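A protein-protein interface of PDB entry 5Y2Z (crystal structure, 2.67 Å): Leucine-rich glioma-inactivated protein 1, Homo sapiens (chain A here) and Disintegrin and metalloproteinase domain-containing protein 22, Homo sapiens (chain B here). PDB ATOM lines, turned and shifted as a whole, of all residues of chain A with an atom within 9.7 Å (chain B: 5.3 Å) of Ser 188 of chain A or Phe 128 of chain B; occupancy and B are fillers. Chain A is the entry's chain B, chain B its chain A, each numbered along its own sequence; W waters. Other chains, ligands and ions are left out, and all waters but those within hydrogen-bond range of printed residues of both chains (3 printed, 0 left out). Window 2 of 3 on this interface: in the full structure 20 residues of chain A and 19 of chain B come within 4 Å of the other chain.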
ATOM      1  N   LYS A 136     -18.711  -7.326  14.124  1.00  0.00           N
ATOM      2  CA  LYS A 136     -17.417  -7.935  14.411  1.00  0.00           C
ATOM      3  C   LYS A 136     -16.531  -7.069  15.309  1.00  0.00           C
ATOM      4  O   LYS A 136     -15.939  -7.568  16.269  1.00  0.00           O
ATOM      5  CB  LYS A 136     -16.690  -8.244  13.109  1.00  0.00           C
ATOM      6  CG  LYS A 136     -16.746  -9.713  12.724  1.00  0.00           C
ATOM      7  CD  LYS A 136     -15.687 -10.061  11.693  1.00  0.00           C
ATOM      8  CE  LYS A 136     -15.402 -11.553  11.676  1.00  0.00           C
ATOM      9  NZ  LYS A 136     -14.283 -11.882  10.748  1.00  0.00           N
ATOM     10  N   HIS A 157     -16.366 -13.341  23.306  1.00  0.00           N
ATOM     11  CA  HIS A 157     -16.564 -13.701  21.906  1.00  0.00           C
ATOM     12  C   HIS A 157     -16.111 -12.619  20.922  1.00  0.00           C
ATOM     13  O   HIS A 157     -16.922 -12.048  20.189  1.00  0.00           O
ATOM     14  CB  HIS A 157     -18.041 -14.035  21.667  1.00  0.00           C
ATOM     15  CG  HIS A 157     -18.276 -15.439  21.207  1.00  0.00           C
ATOM     16  ND1 HIS A 157     -19.363 -15.798  20.437  1.00  0.00           N
ATOM     17  CD2 HIS A 157     -17.558 -16.572  21.397  1.00  0.00           C
ATOM     18  CE1 HIS A 157     -19.303 -17.091  20.174  1.00  0.00           C
ATOM     19  NE2 HIS A 157     -18.218 -17.583  20.744  1.00  0.00           N
ATOM     20  N   TRP A 159     -14.720 -10.757  17.698  1.00  0.00           N
ATOM     21  CA  TRP A 159     -14.899 -10.925  16.248  1.00  0.00           C
ATOM     22  C   TRP A 159     -16.084 -11.830  15.892  1.00  0.00           C
ATOM     23  O   TRP A 159     -16.208 -12.297  14.761  1.00  0.00           O
ATOM     24  CB  TRP A 159     -13.618 -11.473  15.593  1.00  0.00           C
ATOM     25  CG  TRP A 159     -12.337 -10.956  16.191  1.00  0.00           C
ATOM     26  CD1 TRP A 159     -11.365 -11.692  16.806  1.00  0.00           C
ATOM     27  CD2 TRP A 159     -11.902  -9.592  16.245  1.00  0.00           C
ATOM     28  NE1 TRP A 159     -10.350 -10.873  17.230  1.00  0.00           N
ATOM     29  CE2 TRP A 159     -10.653  -9.578  16.899  1.00  0.00           C
ATOM     30  CE3 TRP A 159     -12.447  -8.380  15.805  1.00  0.00           C
ATOM     31  CZ2 TRP A 159      -9.938  -8.400  17.119  1.00  0.00           C
ATOM     32  CZ3 TRP A 159     -11.735  -7.211  16.025  1.00  0.00           C
ATOM     33  CH2 TRP A 159     -10.495  -7.231  16.677  1.00  0.00           C
ATOM     34  N   TYR A 160     -16.968 -12.041  16.858  1.00  0.00           N
ATOM     35  CA  TYR A 160     -18.160 -12.862  16.676  1.00  0.00           C
ATOM     36  C   TYR A 160     -19.422 -12.014  16.528  1.00  0.00           C
ATOM     37  O   TYR A 160     -19.560 -10.975  17.169  1.00  0.00           O
ATOM     38  CB  TYR A 160     -18.283 -13.823  17.855  1.00  0.00           C
ATOM     39  CG  TYR A 160     -17.476 -15.092  17.688  1.00  0.00           C
ATOM     40  CD1 TYR A 160     -17.612 -15.878  16.556  1.00  0.00           C
ATOM     41  CD2 TYR A 160     -16.506 -15.443  18.609  1.00  0.00           C
ATOM     42  CE1 TYR A 160     -16.865 -17.026  16.391  1.00  0.00           C
ATOM     43  CE2 TYR A 160     -15.750 -16.586  18.454  1.00  0.00           C
ATOM     44  CZ  TYR A 160     -15.930 -17.372  17.340  1.00  0.00           C
ATOM     45  OH  TYR A 160     -15.175 -18.509  17.177  1.00  0.00           O
ATOM     46  N   ARG A 161     -20.326 -12.449  15.657  1.00  0.00           N
ATOM     47  CA  ARG A 161     -21.584 -11.745  15.449  1.00  0.00           C
ATOM     48  C   ARG A 161     -22.647 -12.249  16.410  1.00  0.00           C
ATOM     49  O   ARG A 161     -23.599 -12.914  16.001  1.00  0.00           O
ATOM     50  CB  ARG A 161     -22.052 -11.900  14.000  1.00  0.00           C
ATOM     51  CG  ARG A 161     -21.110 -11.265  12.977  1.00  0.00           C
ATOM     52  CD  ARG A 161     -21.701 -11.285  11.572  1.00  0.00           C
ATOM     53  NE  ARG A 161     -21.274 -10.129  10.788  1.00  0.00           N
ATOM     54  CZ  ARG A 161     -20.224 -10.120   9.974  1.00  0.00           C
ATOM     55  NH1 ARG A 161     -19.483 -11.208   9.832  1.00  0.00           N
ATOM     56  NH2 ARG A 161     -19.916  -9.019   9.303  1.00  0.00           N
ATOM     57  N   ASP A 162     -22.489 -11.918  17.688  1.00  0.00           N
ATOM     58  CA  ASP A 162     -23.384 -12.424  18.714  1.00  0.00           C
ATOM     59  C   ASP A 162     -24.789 -11.855  18.557  1.00  0.00           C
ATOM     60  O   ASP A 162     -24.979 -10.646  18.450  1.00  0.00           O
ATOM     61  CB  ASP A 162     -22.832 -12.118  20.103  1.00  0.00           C
ATOM     62  CG  ASP A 162     -21.474 -12.746  20.334  1.00  0.00           C
ATOM     63  OD1 ASP A 162     -21.404 -13.986  20.479  1.00  0.00           O
ATOM     64  OD2 ASP A 162     -20.474 -12.000  20.367  1.00  0.00           O
ATOM     65  N   THR A 163     -25.769 -12.746  18.550  1.00  0.00           N
ATOM     66  CA  THR A 163     -27.155 -12.367  18.339  1.00  0.00           C
ATOM     67  C   THR A 163     -27.945 -12.274  19.642  1.00  0.00           C
ATOM     68  O   THR A 163     -28.730 -11.345  19.834  1.00  0.00           O
ATOM     69  CB  THR A 163     -27.844 -13.356  17.401  1.00  0.00           C
ATOM     70  OG1 THR A 163     -27.386 -13.129  16.062  1.00  0.00           O
ATOM     71  CG2 THR A 163     -29.321 -13.136  17.422  1.00  0.00           C
ATOM     72  N   LEU A 184     -24.093 -17.677  24.537  1.00  0.00           N
ATOM     73  CA  LEU A 184     -24.040 -16.764  23.400  1.00  0.00           C
ATOM     74  C   LEU A 184     -24.382 -17.457  22.082  1.00  0.00           C
ATOM     75  O   LEU A 184     -23.844 -18.517  21.766  1.00  0.00           O
ATOM     76  CB  LEU A 184     -22.662 -16.112  23.290  1.00  0.00           C
ATOM     77  CG  LEU A 184     -22.343 -15.050  24.337  1.00  0.00           C
ATOM     78  CD1 LEU A 184     -20.991 -14.407  24.062  1.00  0.00           C
ATOM     79  CD2 LEU A 184     -23.446 -14.006  24.375  1.00  0.00           C
ATOM     80  N   SER A 185     -25.274 -16.835  21.316  1.00  0.00           N
ATOM     81  CA  SER A 185     -25.648 -17.321  19.993  1.00  0.00           C
ATOM     82  C   SER A 185     -25.117 -16.364  18.934  1.00  0.00           C
ATOM     83  O   SER A 185     -25.343 -15.159  19.015  1.00  0.00           O
ATOM     84  CB  SER A 185     -27.168 -17.449  19.867  1.00  0.00           C
ATOM     85  OG  SER A 185     -27.704 -18.314  20.854  1.00  0.00           O
ATOM     86  N   SER A 186     -24.404 -16.896  17.946  1.00  0.00           N
ATOM     87  CA  SER A 186     -23.834 -16.067  16.889  1.00  0.00           C
ATOM     88  C   SER A 186     -24.120 -16.621  15.490  1.00  0.00           C
ATOM     89  O   SER A 186     -24.371 -17.814  15.330  1.00  0.00           O
ATOM     90  CB  SER A 186     -22.327 -15.922  17.105  1.00  0.00           C
ATOM     91  OG  SER A 186     -21.753 -17.156  17.499  1.00  0.00           O
ATOM     92  N   SER A 187     -24.063 -15.751  14.482  1.00  0.00           N
ATOM     93  CA  SER A 187     -24.378 -16.125  13.101  1.00  0.00           C
ATOM     94  C   SER A 187     -23.447 -17.196  12.550  1.00  0.00           C
ATOM     95  O   SER A 187     -22.224 -17.098  12.671  1.00  0.00           O
ATOM     96  CB  SER A 187     -24.339 -14.902  12.177  1.00  0.00           C
ATOM     97  OG  SER A 187     -25.386 -13.995  12.474  1.00  0.00           O
ATOM     98  N   SER A 188     -24.047 -18.218  11.942  1.00  0.00           N
ATOM     99  CA  SER A 188     -23.311 -19.324  11.338  1.00  0.00           C
ATOM    100  C   SER A 188     -22.340 -19.956  12.329  1.00  0.00           C
ATOM    101  O   SER A 188     -21.228 -20.331  11.970  1.00  0.00           O
ATOM    102  CB  SER A 188     -22.556 -18.844  10.095  1.00  0.00           C
ATOM    103  OG  SER A 188     -23.455 -18.478   9.062  1.00  0.00           O
ATOM    104  N   GLN A 189     -22.771 -20.076  13.578  1.00  0.00           N
ATOM    105  CA  GLN A 189     -21.893 -20.553  14.633  1.00  0.00           C
ATOM    106  C   GLN A 189     -22.671 -21.330  15.695  1.00  0.00           C
ATOM    107  O   GLN A 189     -23.894 -21.237  15.778  1.00  0.00           O
ATOM    108  CB  GLN A 189     -21.142 -19.372  15.256  1.00  0.00           C
ATOM    109  CG  GLN A 189     -19.761 -19.717  15.766  1.00  0.00           C
ATOM    110  CD  GLN A 189     -18.791 -20.044  14.649  1.00  0.00           C
ATOM    111  OE1 GLN A 189     -17.916 -20.894  14.803  1.00  0.00           O
ATOM    112  NE2 GLN A 189     -18.935 -19.361  13.519  1.00  0.00           N
ATOM    113  N   ARG A 190     -21.953 -22.120  16.483  1.00  0.00           N
ATOM    114  CA  ARG A 190     -22.551 -22.894  17.564  1.00  0.00           C
ATOM    115  C   ARG A 190     -22.730 -22.046  18.824  1.00  0.00           C
ATOM    116  O   ARG A 190     -21.918 -21.161  19.098  1.00  0.00           O
ATOM    117  CB  ARG A 190     -21.680 -24.112  17.881  1.00  0.00           C
ATOM    118  CG  ARG A 190     -22.030 -25.362  17.107  1.00  0.00           C
ATOM    119  CD  ARG A 190     -20.933 -26.399  17.193  1.00  0.00           C
ATOM    120  NE  ARG A 190     -19.761 -26.001  16.424  1.00  0.00           N
ATOM    121  CZ  ARG A 190     -18.533 -26.447  16.658  1.00  0.00           C
ATOM    122  NH1 ARG A 190     -18.317 -27.290  17.658  1.00  0.00           N
ATOM    123  NH2 ARG A 190     -17.522 -26.037  15.902  1.00  0.00           N
ATOM    124  N   PRO A 191     -23.807 -22.302  19.582  1.00  0.00           N
ATOM    125  CA  PRO A 191     -24.034 -21.643  20.872  1.00  0.00           C
ATOM    126  C   PRO A 191     -22.910 -21.940  21.858  1.00  0.00           C
ATOM    127  O   PRO A 191     -22.433 -23.074  21.922  1.00  0.00           O
ATOM    128  CB  PRO A 191     -25.354 -22.250  21.351  1.00  0.00           C
ATOM    129  CG  PRO A 191     -26.040 -22.691  20.107  1.00  0.00           C
ATOM    130  CD  PRO A 191     -24.945 -23.153  19.193  1.00  0.00           C
ATOM    131  N   MET A 212     -25.999 -28.101  17.169  1.00  0.00           N
ATOM    132  CA  MET A 212     -26.698 -26.873  16.844  1.00  0.00           C
ATOM    133  C   MET A 212     -25.856 -25.954  15.986  1.00  0.00           C
ATOM    134  O   MET A 212     -24.867 -25.409  16.441  1.00  0.00           O
ATOM    135  CB  MET A 212     -27.084 -26.133  18.125  1.00  0.00           C
ATOM    136  CG  MET A 212     -28.081 -26.868  18.999  1.00  0.00           C
ATOM    137  SD  MET A 212     -29.550 -27.438  18.119  1.00  0.00           S
ATOM    138  CE  MET A 212     -30.483 -25.939  17.853  1.00  0.00           C
ATOM    139  N   GLU A 213     -26.296 -25.730  14.757  1.00  0.00           N
ATOM    140  CA  GLU A 213     -25.579 -24.847  13.872  1.00  0.00           C
ATOM    141  C   GLU A 213     -26.543 -23.713  13.546  1.00  0.00           C
ATOM    142  O   GLU A 213     -27.717 -23.963  13.270  1.00  0.00           O
ATOM    143  CB  GLU A 213     -25.164 -25.590  12.599  1.00  0.00           C
ATOM    144  CG  GLU A 213     -24.278 -26.839  12.803  1.00  0.00           C
ATOM    145  CD  GLU A 213     -23.019 -26.605  13.621  1.00  0.00           C
ATOM    146  OE1 GLU A 213     -22.463 -27.600  14.137  1.00  0.00           O
ATOM    147  OE2 GLU A 213     -22.572 -25.445  13.738  1.00  0.00           O
ATOM    148  N   ASP A 214     -26.054 -22.474  13.573  1.00  0.00           N
ATOM    149  CA  ASP A 214     -26.857 -21.309  13.195  1.00  0.00           C
ATOM    150  C   ASP A 214     -28.026 -20.981  14.145  1.00  0.00           C
ATOM    151  O   ASP A 214     -29.046 -20.444  13.705  1.00  0.00           O
ATOM    152  CB  ASP A 214     -27.388 -21.462  11.770  1.00  0.00           C
ATOM    153  CG  ASP A 214     -27.438 -20.144  11.029  1.00  0.00           C
ATOM    154  OD1 ASP A 214     -27.207 -19.094  11.674  1.00  0.00           O
ATOM    155  OD2 ASP A 214     -27.700 -20.159   9.808  1.00  0.00           O
ATOM    156  N   VAL A 215     -27.895 -21.316  15.425  1.00  0.00           N
ATOM    157  CA  VAL A 215     -28.928 -20.978  16.404  1.00  0.00           C
ATOM    158  C   VAL A 215     -29.020 -19.472  16.594  1.00  0.00           C
ATOM    159  O   VAL A 215     -28.005 -18.792  16.736  1.00  0.00           O
ATOM    160  CB  VAL A 215     -28.653 -21.633  17.759  1.00  0.00           C
ATOM    161  CG1 VAL A 215     -29.743 -21.270  18.766  1.00  0.00           C
ATOM    162  CG2 VAL A 215     -28.588 -23.112  17.581  1.00  0.00           C
ATOM    163  N   TYR A 216     -30.243 -18.954  16.571  1.00  0.00           N
ATOM    164  CA  TYR A 216     -30.469 -17.520  16.697  1.00  0.00           C
ATOM    165  C   TYR A 216     -30.496 -17.045  18.152  1.00  0.00           C
ATOM    166  O   TYR A 216     -29.890 -16.032  18.485  1.00  0.00           O
ATOM    167  CB  TYR A 216     -31.779 -17.130  16.005  1.00  0.00           C
ATOM    168  CG  TYR A 216     -32.082 -15.653  16.084  1.00  0.00           C
ATOM    169  CD1 TYR A 216     -31.488 -14.760  15.205  1.00  0.00           C
ATOM    170  CD2 TYR A 216     -32.967 -15.152  17.031  1.00  0.00           C
ATOM    171  CE1 TYR A 216     -31.763 -13.408  15.265  1.00  0.00           C
ATOM    172  CE2 TYR A 216     -33.241 -13.799  17.103  1.00  0.00           C
ATOM    173  CZ  TYR A 216     -32.634 -12.932  16.220  1.00  0.00           C
ATOM    174  OH  TYR A 216     -32.903 -11.586  16.286  1.00  0.00           O
ATOM    175  N   ARG A 233     -34.361 -21.451  15.554  1.00  0.00           N
ATOM    176  CA  ARG A 233     -33.827 -21.170  14.231  1.00  0.00           C
ATOM    177  C   ARG A 233     -34.837 -20.472  13.358  1.00  0.00           C
ATOM    178  O   ARG A 233     -36.041 -20.582  13.570  1.00  0.00           O
ATOM    179  CB  ARG A 233     -33.363 -22.424  13.514  1.00  0.00           C
ATOM    180  CG  ARG A 233     -32.002 -22.863  13.922  1.00  0.00           C
ATOM    181  CD  ARG A 233     -31.485 -23.896  12.957  1.00  0.00           C
ATOM    182  NE  ARG A 233     -30.212 -24.402  13.427  1.00  0.00           N
ATOM    183  CZ  ARG A 233     -30.118 -25.406  14.286  1.00  0.00           C
ATOM    184  NH1 ARG A 233     -31.217 -25.987  14.735  1.00  0.00           N
ATOM    185  NH2 ARG A 233     -28.942 -25.830  14.694  1.00  0.00           N
ATOM    186  N   MET B  19     -14.641 -23.967   3.102  1.00  0.00           N
ATOM    187  CA  MET B  19     -15.916 -23.618   2.490  1.00  0.00           C
ATOM    188  C   MET B  19     -16.572 -24.884   1.960  1.00  0.00           C
ATOM    189  O   MET B  19     -17.785 -25.044   2.032  1.00  0.00           O
ATOM    190  CB  MET B  19     -15.710 -22.588   1.371  1.00  0.00           C
ATOM    191  CG  MET B  19     -16.956 -22.168   0.609  1.00  0.00           C
ATOM    192  SD  MET B  19     -18.141 -21.168   1.527  1.00  0.00           S
ATOM    193  CE  MET B  19     -17.159 -19.750   1.976  1.00  0.00           C
ATOM    194  N   LYS B  22     -18.035 -26.838   4.820  1.00  0.00           N
ATOM    195  CA  LYS B  22     -19.262 -26.214   5.304  1.00  0.00           C
ATOM    196  C   LYS B  22     -20.475 -26.694   4.514  1.00  0.00           C
ATOM    197  O   LYS B  22     -21.587 -26.750   5.037  1.00  0.00           O
ATOM    198  CB  LYS B  22     -19.158 -24.689   5.229  1.00  0.00           C
ATOM    199  CG  LYS B  22     -18.407 -24.053   6.387  1.00  0.00           C
ATOM    200  CD  LYS B  22     -19.239 -24.064   7.655  1.00  0.00           C
ATOM    201  CE  LYS B  22     -18.455 -23.511   8.835  1.00  0.00           C
ATOM    202  NZ  LYS B  22     -19.163 -23.759  10.126  1.00  0.00           N
ATOM    203  N   HIS B  23     -20.258 -27.065   3.259  1.00  0.00           N
ATOM    204  CA  HIS B  23     -21.350 -27.548   2.432  1.00  0.00           C
ATOM    205  C   HIS B  23     -21.303 -29.063   2.312  1.00  0.00           C
ATOM    206  O   HIS B  23     -21.695 -29.630   1.294  1.00  0.00           O
ATOM    207  CB  HIS B  23     -21.310 -26.888   1.059  1.00  0.00           C
ATOM    208  CG  HIS B  23     -21.428 -25.399   1.115  1.00  0.00           C
ATOM    209  ND1 HIS B  23     -20.343 -24.561   0.980  1.00  0.00           N
ATOM    210  CD2 HIS B  23     -22.498 -24.597   1.330  1.00  0.00           C
ATOM    211  CE1 HIS B  23     -20.743 -23.307   1.087  1.00  0.00           C
ATOM    212  NE2 HIS B  23     -22.046 -23.301   1.304  1.00  0.00           N
ATOM    213  N   TYR B  33     -24.544 -22.201  -3.767  1.00  0.00           N
ATOM    214  CA  TYR B  33     -24.445 -21.323  -2.608  1.00  0.00           C
ATOM    215  C   TYR B  33     -23.660 -20.072  -2.965  1.00  0.00           C
ATOM    216  O   TYR B  33     -24.050 -18.961  -2.598  1.00  0.00           O
ATOM    217  CB  TYR B  33     -23.778 -22.045  -1.438  1.00  0.00           C
ATOM    218  CG  TYR B  33     -23.824 -21.291  -0.128  1.00  0.00           C
ATOM    219  CD1 TYR B  33     -22.826 -20.388   0.213  1.00  0.00           C
ATOM    220  CD2 TYR B  33     -24.854 -21.503   0.780  1.00  0.00           C
ATOM    221  CE1 TYR B  33     -22.861 -19.710   1.414  1.00  0.00           C
ATOM    222  CE2 TYR B  33     -24.897 -20.829   1.981  1.00  0.00           C
ATOM    223  CZ  TYR B  33     -23.900 -19.934   2.294  1.00  0.00           C
ATOM    224  OH  TYR B  33     -23.944 -19.258   3.493  1.00  0.00           O
ATOM    225  N   SER B  99     -13.869 -18.075   1.833  1.00  0.00           N
ATOM    226  CA  SER B  99     -13.306 -18.868   2.920  1.00  0.00           C
ATOM    227  C   SER B  99     -14.385 -19.331   3.893  1.00  0.00           C
ATOM    228  O   SER B  99     -15.237 -18.547   4.297  1.00  0.00           O
ATOM    229  CB  SER B  99     -12.240 -18.077   3.672  1.00  0.00           C
ATOM    230  OG  SER B  99     -11.673 -18.863   4.706  1.00  0.00           O
ATOM    231  N   GLY B 100     -14.350 -20.607   4.261  1.00  0.00           N
ATOM    232  CA  GLY B 100     -15.303 -21.150   5.211  1.00  0.00           C
ATOM    233  C   GLY B 100     -14.981 -20.740   6.636  1.00  0.00           C
ATOM    234  O   GLY B 100     -15.800 -20.889   7.547  1.00  0.00           O
ATOM    235  N   SER B 101     -13.777 -20.216   6.826  1.00  0.00           N
ATOM    236  CA  SER B 101     -13.325 -19.786   8.141  1.00  0.00           C
ATOM    237  C   SER B 101     -13.873 -18.412   8.514  1.00  0.00           C
ATOM    238  O   SER B 101     -14.644 -17.806   7.767  1.00  0.00           O
ATOM    239  CB  SER B 101     -11.794 -19.773   8.194  1.00  0.00           C
ATOM    240  OG  SER B 101     -11.262 -18.749   7.374  1.00  0.00           O
ATOM    241  N   ASN B 126     -13.179 -13.115   1.261  1.00  0.00           N
ATOM    242  CA  ASN B 126     -14.426 -12.999   2.018  1.00  0.00           C
ATOM    243  C   ASN B 126     -14.685 -14.186   2.951  1.00  0.00           C
ATOM    244  O   ASN B 126     -14.558 -15.340   2.545  1.00  0.00           O
ATOM    245  CB  ASN B 126     -15.607 -12.846   1.059  1.00  0.00           C
ATOM    246  CG  ASN B 126     -15.409 -11.720   0.064  1.00  0.00           C
ATOM    247  OD1 ASN B 126     -15.751 -10.568   0.334  1.00  0.00           O
ATOM    248  ND2 ASN B 126     -14.859 -12.048  -1.099  1.00  0.00           N
ATOM    249  N   GLU B 127     -15.067 -13.904   4.194  1.00  0.00           N
ATOM    250  CA  GLU B 127     -15.318 -14.967   5.163  1.00  0.00           C
ATOM    251  C   GLU B 127     -16.723 -15.537   5.023  1.00  0.00           C
ATOM    252  O   GLU B 127     -17.618 -14.900   4.472  1.00  0.00           O
ATOM    253  CB  GLU B 127     -15.124 -14.460   6.592  1.00  0.00           C
ATOM    254  CG  GLU B 127     -16.289 -13.628   7.107  1.00  0.00           C
ATOM    255  CD  GLU B 127     -16.117 -13.203   8.555  1.00  0.00           C
ATOM    256  OE1 GLU B 127     -15.045 -13.483   9.133  1.00  0.00           O
ATOM    257  OE2 GLU B 127     -17.054 -12.583   9.113  1.00  0.00           O
ATOM    258  N   PHE B 128     -16.919 -16.733   5.563  1.00  0.00           N
ATOM    259  CA  PHE B 128     -18.204 -17.404   5.455  1.00  0.00           C
ATOM    260  C   PHE B 128     -19.268 -16.714   6.301  1.00  0.00           C
ATOM    261  O   PHE B 128     -18.971 -16.112   7.331  1.00  0.00           O
ATOM    262  CB  PHE B 128     -18.080 -18.873   5.870  1.00  0.00           C
ATOM    263  CG  PHE B 128     -19.374 -19.628   5.796  1.00  0.00           C
ATOM    264  CD1 PHE B 128     -19.868 -20.061   4.578  1.00  0.00           C
ATOM    265  CD2 PHE B 128     -20.102 -19.897   6.942  1.00  0.00           C
ATOM    266  CE1 PHE B 128     -21.065 -20.748   4.505  1.00  0.00           C
ATOM    267  CE2 PHE B 128     -21.298 -20.585   6.874  1.00  0.00           C
ATOM    268  CZ  PHE B 128     -21.780 -21.010   5.655  1.00  0.00           C
ATOM    269  N   GLY B 129     -20.512 -16.816   5.852  1.00  0.00           N
ATOM    270  CA  GLY B 129     -21.649 -16.274   6.567  1.00  0.00           C
ATOM    271  C   GLY B 129     -22.938 -16.720   5.909  1.00  0.00           C
ATOM    272  O   GLY B 129     -22.919 -17.509   4.962  1.00  0.00           O
ATOM    273  N   LYS B 130     -24.064 -16.223   6.406  1.00  0.00           N
ATOM    274  CA  LYS B 130     -25.347 -16.505   5.778  1.00  0.00           C
ATOM    275  C   LYS B 130     -25.354 -15.880   4.387  1.00  0.00           C
ATOM    276  O   LYS B 130     -24.630 -14.921   4.137  1.00  0.00           O
ATOM    277  CB  LYS B 130     -26.483 -15.957   6.635  1.00  0.00           C
ATOM    278  CG  LYS B 130     -26.631 -16.658   7.979  1.00  0.00           C
ATOM    279  CD  LYS B 130     -27.771 -16.065   8.793  1.00  0.00           C
ATOM    280  CE  LYS B 130     -29.123 -16.417   8.206  1.00  0.00           C
ATOM    281  NZ  LYS B 130     -30.225 -15.904   9.064  1.00  0.00           N
ATOM    282  N   MET B 134     -23.029 -12.637   3.393  1.00  0.00           N
ATOM    283  CA  MET B 134     -21.816 -12.745   2.595  1.00  0.00           C
ATOM    284  C   MET B 134     -21.933 -11.928   1.315  1.00  0.00           C
ATOM    285  O   MET B 134     -20.931 -11.448   0.785  1.00  0.00           O
ATOM    286  CB  MET B 134     -21.507 -14.205   2.257  1.00  0.00           C
ATOM    287  CG  MET B 134     -20.024 -14.469   2.117  1.00  0.00           C
ATOM    288  SD  MET B 134     -19.649 -16.154   1.620  1.00  0.00           S
ATOM    289  CE  MET B 134     -20.714 -17.085   2.701  1.00  0.00           C
HETATM  290  O   HOH W   1     -21.044 -23.679  12.882  1.00  0.00           O
HETATM  291  O   HOH W   2     -23.418 -15.791   8.851  1.00  0.00           O
HETATM  292  O   HOH W   3     -18.359 -13.758  11.781  1.00  0.00           O
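OE2 of Glu 127 of chain B is in salt-bridge range of NZ of Lys 136 of chain A (3.3 Å).
OE2 of Glu 127 of chain B lies within salt-bridge range of NH1 of Arg 161 of chain A (2.9 Å).
The side-chain hydroxyl (OH) of Tyr 33 of chain B is in hydrogen-bond range of the backbone carbonyl oxygen (O) of Gly 129 of chain B (2.5 Å).
The backbone carbonyl oxygen (O) of Ser 99 of chain B is in hydrogen-bond range of the backbone NH (N) of Phe 128 of chain B.
The backbone NH of Phe 128 of chain B is in hydrogen-bond range of the backbone carbonyl oxygen of Ser 101 of chain B (3.3 Å).
The backbone carbonyl oxygen of Arg 161 of chain A lies within hydrogen-bond range of the backbone NH of Ser 187 of chain A (3.3 Å).
N of Ser 188 of chain A lies within hydrogen-bond range of OD1 of Asp 214 of chain A (3.3 Å).
Among the printed residues, merely in contact across the chains: Ser 188 of chain A with Lys 130 of chain B, Ser 188 of chain A with Gly 129 of chain B and Ser 188 of chain A with Phe 128 of chain B.
Phe 128 of chain B touches one residue of chain A.
No residue of chain A comes within 4 Å of Gly 100 of chain B.
Gly 129 of chain B touches just one residue of chain A: Ser 188.
Printed residues of chain B within 4 Å of Lys 136 of chain A: Glu 127 (2.4 Å).
Printed residues of chain A within 4 Å of Lys 130 of chain B: Ser 188.
Ser 186 of chain A touches none of the printed residues of chain B.
The nearest residue of chain B that does not touch Ser 188 of chain A is Lys 22 of chain B (4.4 Å).
The nearest residue of chain A that does not touch Phe 128 of chain B is Arg 161 of chain A (5.5 Å).
The nearest printed residue of chain A that does not touch Lys 130 of chain B is Asp 214 of chain A (4.1 Å).
Of the 13 printed residues of chain B, 4 touch a printed residue of chain A.
Along chain A the printed residues that touch a printed residue of chain B span positions 136 to 188.
Among the printed residues, 5 pairs touch across the chains.
Among the printed residues, Asp or Glu carboxylates within 4 Å of a Lys or Arg side-chain nitrogen of the other chain: Lys 136 of chain A with Glu 127 of chain B (2.4 Å) and Arg 161 of chain A with Glu 127 of chain B (2.9 Å).
Water W1 lies within hydrogen-bond range of the side-chain carboxylate (OE2) of Glu 213 of chain A (2.5 Å), the side-chain amino group (NZ) of Lys 22 of chain B (3.3 Å) and the backbone carbonyl oxygen (O) of Ser 188 of chain A (3.5 Å).
Water W2 lies within hydrogen-bond range of N of Lys 130 of chain B and OG of Ser 188 of chain A.
Water W3 lies within hydrogen-bond range of OE2 of Glu 127 of chain B (3.2 Å) and NH1 of Arg 161 of chain A (3.4 Å).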
